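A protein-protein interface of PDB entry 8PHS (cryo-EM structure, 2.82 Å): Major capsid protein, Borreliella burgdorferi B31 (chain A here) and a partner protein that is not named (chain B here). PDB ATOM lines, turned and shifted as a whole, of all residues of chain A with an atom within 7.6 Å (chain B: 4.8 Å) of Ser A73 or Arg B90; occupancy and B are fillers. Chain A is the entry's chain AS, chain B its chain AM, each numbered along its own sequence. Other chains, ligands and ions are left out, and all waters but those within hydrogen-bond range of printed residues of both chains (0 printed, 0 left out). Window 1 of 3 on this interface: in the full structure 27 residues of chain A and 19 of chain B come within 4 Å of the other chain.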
ATOM      1  N   VAL A  47      15.363  19.476  10.955  1.00  0.00           N
ATOM      2  CA  VAL A  47      15.147  18.695   9.742  1.00  0.00           C
ATOM      3  C   VAL A  47      16.473  18.083   9.319  1.00  0.00           C
ATOM      4  O   VAL A  47      17.478  18.791   9.188  1.00  0.00           O
ATOM      5  CB  VAL A  47      14.557  19.556   8.613  1.00  0.00           C
ATOM      6  CG1 VAL A  47      14.154  18.682   7.438  1.00  0.00           C
ATOM      7  CG2 VAL A  47      13.373  20.361   9.120  1.00  0.00           C
ATOM      8  N   LYS A  48      16.476  16.770   9.107  1.00  0.00           N
ATOM      9  CA  LYS A  48      17.650  16.045   8.643  1.00  0.00           C
ATOM     10  C   LYS A  48      17.378  15.481   7.257  1.00  0.00           C
ATOM     11  O   LYS A  48      16.380  14.781   7.053  1.00  0.00           O
ATOM     12  CB  LYS A  48      18.017  14.922   9.614  1.00  0.00           C
ATOM     13  CG  LYS A  48      19.169  14.048   9.157  1.00  0.00           C
ATOM     14  CD  LYS A  48      19.285  12.812  10.033  1.00  0.00           C
ATOM     15  CE  LYS A  48      20.359  11.867   9.524  1.00  0.00           C
ATOM     16  NZ  LYS A  48      20.392  10.599  10.304  1.00  0.00           N
ATOM     17  N   TRP A  49      18.264  15.780   6.315  1.00  0.00           N
ATOM     18  CA  TRP A  49      18.105  15.374   4.928  1.00  0.00           C
ATOM     19  C   TRP A  49      19.037  14.213   4.606  1.00  0.00           C
ATOM     20  O   TRP A  49      20.151  14.124   5.128  1.00  0.00           O
ATOM     21  CB  TRP A  49      18.386  16.542   3.981  1.00  0.00           C
ATOM     22  CG  TRP A  49      17.354  17.620   4.042  1.00  0.00           C
ATOM     23  CD1 TRP A  49      17.415  18.773   4.765  1.00  0.00           C
ATOM     24  CD2 TRP A  49      16.099  17.643   3.355  1.00  0.00           C
ATOM     25  NE1 TRP A  49      16.279  19.516   4.568  1.00  0.00           N
ATOM     26  CE2 TRP A  49      15.454  18.843   3.706  1.00  0.00           C
ATOM     27  CE3 TRP A  49      15.458  16.765   2.476  1.00  0.00           C
ATOM     28  CZ2 TRP A  49      14.201  19.190   3.209  1.00  0.00           C
ATOM     29  CZ3 TRP A  49      14.216  17.112   1.982  1.00  0.00           C
ATOM     30  CH2 TRP A  49      13.600  18.313   2.351  1.00  0.00           C
ATOM     31  N   ASP A  50      18.564  13.320   3.739  1.00  0.00           N
ATOM     32  CA  ASP A  50      19.329  12.153   3.325  1.00  0.00           C
ATOM     33  C   ASP A  50      19.118  11.916   1.838  1.00  0.00           C
ATOM     34  O   ASP A  50      18.188  12.445   1.227  1.00  0.00           O
ATOM     35  CB  ASP A  50      18.932  10.900   4.116  1.00  0.00           C
ATOM     36  CG  ASP A  50      18.951  11.125   5.613  1.00  0.00           C
ATOM     37  OD1 ASP A  50      20.046  11.366   6.166  1.00  0.00           O
ATOM     38  OD2 ASP A  50      17.872  11.059   6.239  1.00  0.00           O
ATOM     39  N   ALA A  51      20.003  11.109   1.259  1.00  0.00           N
ATOM     40  CA  ALA A  51      19.914  10.721  -0.139  1.00  0.00           C
ATOM     41  C   ALA A  51      20.168   9.227  -0.255  1.00  0.00           C
ATOM     42  O   ALA A  51      20.857   8.634   0.578  1.00  0.00           O
ATOM     43  CB  ALA A  51      20.911  11.495  -1.008  1.00  0.00           C
ATOM     44  N   PHE A  52      19.600   8.620  -1.294  1.00  0.00           N
ATOM     45  CA  PHE A  52      19.742   7.190  -1.522  1.00  0.00           C
ATOM     46  C   PHE A  52      19.810   6.915  -3.017  1.00  0.00           C
ATOM     47  O   PHE A  52      19.359   7.721  -3.834  1.00  0.00           O
ATOM     48  CB  PHE A  52      18.590   6.404  -0.876  1.00  0.00           C
ATOM     49  CG  PHE A  52      17.223   6.950  -1.191  1.00  0.00           C
ATOM     50  CD1 PHE A  52      16.661   6.783  -2.445  1.00  0.00           C
ATOM     51  CD2 PHE A  52      16.509   7.645  -0.231  1.00  0.00           C
ATOM     52  CE1 PHE A  52      15.408   7.285  -2.731  1.00  0.00           C
ATOM     53  CE2 PHE A  52      15.257   8.154  -0.513  1.00  0.00           C
ATOM     54  CZ  PHE A  52      14.706   7.974  -1.765  1.00  0.00           C
ATOM     55  N   GLY A  71      17.415   9.615  -5.098  1.00  0.00           N
ATOM     56  CA  GLY A  71      16.316  10.184  -4.353  1.00  0.00           C
ATOM     57  C   GLY A  71      16.779  10.906  -3.096  1.00  0.00           C
ATOM     58  O   GLY A  71      17.945  10.872  -2.718  1.00  0.00           O
ATOM     59  N   PHE A  72      15.828  11.579  -2.456  1.00  0.00           N
ATOM     60  CA  PHE A  72      16.084  12.323  -1.234  1.00  0.00           C
ATOM     61  C   PHE A  72      14.983  12.041  -0.222  1.00  0.00           C
ATOM     62  O   PHE A  72      13.877  11.624  -0.573  1.00  0.00           O
ATOM     63  CB  PHE A  72      16.183  13.829  -1.503  1.00  0.00           C
ATOM     64  CG  PHE A  72      17.281  14.200  -2.455  1.00  0.00           C
ATOM     65  CD1 PHE A  72      18.608  14.096  -2.076  1.00  0.00           C
ATOM     66  CD2 PHE A  72      16.989  14.647  -3.731  1.00  0.00           C
ATOM     67  CE1 PHE A  72      19.620  14.434  -2.949  1.00  0.00           C
ATOM     68  CE2 PHE A  72      17.998  14.984  -4.609  1.00  0.00           C
ATOM     69  CZ  PHE A  72      19.315  14.877  -4.217  1.00  0.00           C
ATOM     70  N   SER A  73      15.304  12.269   1.050  1.00  0.00           N
ATOM     71  CA  SER A  73      14.356  12.050   2.132  1.00  0.00           C
ATOM     72  C   SER A  73      14.603  13.075   3.228  1.00  0.00           C
ATOM     73  O   SER A  73      15.663  13.701   3.293  1.00  0.00           O
ATOM     74  CB  SER A  73      14.459  10.631   2.695  1.00  0.00           C
ATOM     75  OG  SER A  73      13.447  10.397   3.657  1.00  0.00           O
ATOM     76  N   SER A  74      13.604  13.244   4.093  1.00  0.00           N
ATOM     77  CA  SER A  74      13.688  14.184   5.200  1.00  0.00           C
ATOM     78  C   SER A  74      13.030  13.587   6.434  1.00  0.00           C
ATOM     79  O   SER A  74      12.132  12.747   6.334  1.00  0.00           O
ATOM     80  CB  SER A  74      13.024  15.522   4.860  1.00  0.00           C
ATOM     81  OG  SER A  74      11.652  15.346   4.560  1.00  0.00           O
ATOM     82  N   GLU A  75      13.493  14.029   7.600  1.00  0.00           N
ATOM     83  CA  GLU A  75      12.940  13.614   8.881  1.00  0.00           C
ATOM     84  C   GLU A  75      12.987  14.795   9.837  1.00  0.00           C
ATOM     85  O   GLU A  75      13.980  15.526   9.880  1.00  0.00           O
ATOM     86  CB  GLU A  75      13.708  12.419   9.456  1.00  0.00           C
ATOM     87  CG  GLU A  75      13.145  11.884  10.758  1.00  0.00           C
ATOM     88  CD  GLU A  75      14.006  10.789  11.352  1.00  0.00           C
ATOM     89  OE1 GLU A  75      15.010  10.409  10.714  1.00  0.00           O
ATOM     90  OE2 GLU A  75      13.681  10.312  12.459  1.00  0.00           O
ATOM     91  N   LYS B  87      18.491   1.549   1.063  1.00  0.00           N
ATOM     92  CA  LYS B  87      17.888   2.744   1.637  1.00  0.00           C
ATOM     93  C   LYS B  87      16.728   3.281   0.810  1.00  0.00           C
ATOM     94  O   LYS B  87      16.071   4.233   1.242  1.00  0.00           O
ATOM     95  CB  LYS B  87      18.934   3.851   1.809  1.00  0.00           C
ATOM     96  CG  LYS B  87      20.141   3.457   2.637  1.00  0.00           C
ATOM     97  CD  LYS B  87      21.147   4.594   2.695  1.00  0.00           C
ATOM     98  CE  LYS B  87      20.487   5.890   3.138  1.00  0.00           C
ATOM     99  NZ  LYS B  87      21.432   7.037   3.092  1.00  0.00           N
ATOM    100  N   ASN B  88      16.463   2.698  -0.359  1.00  0.00           N
ATOM    101  CA  ASN B  88      15.372   3.146  -1.211  1.00  0.00           C
ATOM    102  C   ASN B  88      14.021   2.563  -0.815  1.00  0.00           C
ATOM    103  O   ASN B  88      13.004   2.956  -1.394  1.00  0.00           O
ATOM    104  CB  ASN B  88      15.693   2.826  -2.678  1.00  0.00           C
ATOM    105  CG  ASN B  88      15.745   1.329  -2.971  1.00  0.00           C
ATOM    106  OD1 ASN B  88      14.909   0.550  -2.515  1.00  0.00           O
ATOM    107  ND2 ASN B  88      16.745   0.925  -3.743  1.00  0.00           N
ATOM    108  N   GLU B  89      13.986   1.640   0.144  1.00  0.00           N
ATOM    109  CA  GLU B  89      12.732   1.024   0.562  1.00  0.00           C
ATOM    110  C   GLU B  89      11.920   1.980   1.426  1.00  0.00           C
ATOM    111  O   GLU B  89      11.763   1.758   2.631  1.00  0.00           O
ATOM    112  CB  GLU B  89      13.001  -0.279   1.316  1.00  0.00           C
ATOM    113  CG  GLU B  89      13.818  -1.288   0.530  1.00  0.00           C
ATOM    114  CD  GLU B  89      13.942  -2.618   1.245  1.00  0.00           C
ATOM    115  OE1 GLU B  89      13.418  -2.741   2.372  1.00  0.00           O
ATOM    116  OE2 GLU B  89      14.563  -3.542   0.679  1.00  0.00           O
ATOM    117  N   ARG B  90      11.405   3.046   0.820  1.00  0.00           N
ATOM    118  CA  ARG B  90      10.584   4.029   1.509  1.00  0.00           C
ATOM    119  C   ARG B  90       9.327   4.281   0.692  1.00  0.00           C
ATOM    120  O   ARG B  90       9.371   4.283  -0.542  1.00  0.00           O
ATOM    121  CB  ARG B  90      11.347   5.341   1.729  1.00  0.00           C
ATOM    122  CG  ARG B  90      12.663   5.168   2.467  1.00  0.00           C
ATOM    123  CD  ARG B  90      13.282   6.507   2.821  1.00  0.00           C
ATOM    124  NE  ARG B  90      12.332   7.372   3.508  1.00  0.00           N
ATOM    125  CZ  ARG B  90      12.469   7.787   4.760  1.00  0.00           C
ATOM    126  NH1 ARG B  90      13.515   7.443   5.492  1.00  0.00           N
ATOM    127  NH2 ARG B  90      11.533   8.569   5.290  1.00  0.00           N
ATOM    128  N   VAL B  91       8.205   4.487   1.384  1.00  0.00           N
ATOM    129  CA  VAL B  91       6.933   4.682   0.693  1.00  0.00           C
ATOM    130  C   VAL B  91       6.962   5.962  -0.134  1.00  0.00           C
ATOM    131  O   VAL B  91       6.375   6.028  -1.221  1.00  0.00           O
ATOM    132  CB  VAL B  91       5.766   4.670   1.700  1.00  0.00           C
ATOM    133  CG1 VAL B  91       5.859   5.847   2.662  1.00  0.00           C
ATOM    134  CG2 VAL B  91       4.432   4.679   0.966  1.00  0.00           C
ATOM    135  N   ASP B  92       7.649   6.995   0.356  1.00  0.00           N
ATOM    136  CA  ASP B  92       7.734   8.274  -0.335  1.00  0.00           C
ATOM    137  C   ASP B  92       9.012   8.404  -1.157  1.00  0.00           C
ATOM    138  O   ASP B  92       9.482   9.521  -1.403  1.00  0.00           O
ATOM    139  CB  ASP B  92       7.622   9.426   0.664  1.00  0.00           C
ATOM    140  CG  ASP B  92       8.604   9.302   1.814  1.00  0.00           C
ATOM    141  OD1 ASP B  92       9.371   8.318   1.845  1.00  0.00           O
ATOM    142  OD2 ASP B  92       8.605  10.191   2.690  1.00  0.00           O
ATOM    143  N   ALA B  93       9.584   7.284  -1.585  1.00  0.00           N
ATOM    144  CA  ALA B  93      10.779   7.323  -2.408  1.00  0.00           C
ATOM    145  C   ALA B  93      10.438   7.799  -3.815  1.00  0.00           C
ATOM    146  O   ALA B  93       9.277   7.818  -4.231  1.00  0.00           O
ATOM    147  CB  ALA B  93      11.442   5.947  -2.465  1.00  0.00           C
ATOM    148  N   LYS B 119       1.168   5.950  -6.575  1.00  0.00           N
ATOM    149  CA  LYS B 119       1.821   4.697  -6.960  1.00  0.00           C
ATOM    150  C   LYS B 119       0.803   3.617  -7.323  1.00  0.00           C
ATOM    151  O   LYS B 119       0.930   2.459  -6.922  1.00  0.00           O
ATOM    152  CB  LYS B 119       2.767   4.208  -5.861  1.00  0.00           C
ATOM    153  CG  LYS B 119       4.021   5.055  -5.717  1.00  0.00           C
ATOM    154  CD  LYS B 119       5.039   4.398  -4.802  1.00  0.00           C
ATOM    155  CE  LYS B 119       6.349   5.169  -4.798  1.00  0.00           C
ATOM    156  NZ  LYS B 119       7.367   4.532  -3.921  1.00  0.00           N
ATOM    157  N   ILE B 211       6.841  -2.459   3.946  1.00  0.00           N
ATOM    158  CA  ILE B 211       7.207  -1.335   4.797  1.00  0.00           C
ATOM    159  C   ILE B 211       6.184  -1.271   5.920  1.00  0.00           C
ATOM    160  O   ILE B 211       4.982  -1.123   5.664  1.00  0.00           O
ATOM    161  CB  ILE B 211       7.250  -0.018   4.011  1.00  0.00           C
ATOM    162  CG1 ILE B 211       8.153  -0.164   2.786  1.00  0.00           C
ATOM    163  CG2 ILE B 211       7.723   1.118   4.904  1.00  0.00           C
ATOM    164  CD1 ILE B 211       8.495   1.143   2.121  1.00  0.00           C
ATOM    165  N   LEU B 234       5.460  -3.039  -1.556  1.00  0.00           N
ATOM    166  CA  LEU B 234       5.952  -2.402  -2.766  1.00  0.00           C
ATOM    167  C   LEU B 234       6.800  -3.389  -3.556  1.00  0.00           C
ATOM    168  O   LEU B 234       7.304  -4.379  -3.018  1.00  0.00           O
ATOM    169  CB  LEU B 234       6.775  -1.148  -2.446  1.00  0.00           C
ATOM    170  CG  LEU B 234       6.047   0.005  -1.755  1.00  0.00           C
ATOM    171  CD1 LEU B 234       6.935   1.235  -1.699  1.00  0.00           C
ATOM    172  CD2 LEU B 234       4.742   0.318  -2.463  1.00  0.00           C
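Among the printed residues, merely in contact across the chains: Phe A52 with Lys B87 and Phe A52 with Ala B93.
Trp A49 touches none of the printed residues of chain B. Asp A50 touches none of the printed residues of chain B. Of the printed residues of chain B, Phe A52 touches Lys B87 and Ala B93. Ser A73 touches just one residue of chain B: Arg B90 (3.0 Å). Printed residues of chain A within 4 Å of Lys B87: Ala A51 (3.0 Å) and Phe A52 (3.7 Å). The nearest printed residue of chain B that does not touch Ser A73 is Asp B92 (4.9 Å).
The backbone NH (N) of Ser A73 sits at hydrogen-bond distance from the backbone carbonyl oxygen (O) of Asp A50. The backbone NH (N) of Gly A71 sits at hydrogen-bond distance from the backbone carbonyl oxygen (O) of Phe A52 (3.0 Å). OD1 of Asp B92 is in salt-bridge range of NE of Arg B90 (3.5 Å).
Hydrophobic or aromatic side chains of chain A within 4 Å of the printed part of chain B: Phe A52. Among the printed residues, no Asp or Glu carboxylate lies within 4 Å of a Lys or Arg side-chain nitrogen of the other chain.
The backbone carbonyl oxygen (O) of Ala A51 lies within hydrogen-bond range of the side-chain amino group (NZ) of Lys B87 (3.0 Å). OG of Ser A73 sits close to NH2 of Arg B90 (3.1 Å).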
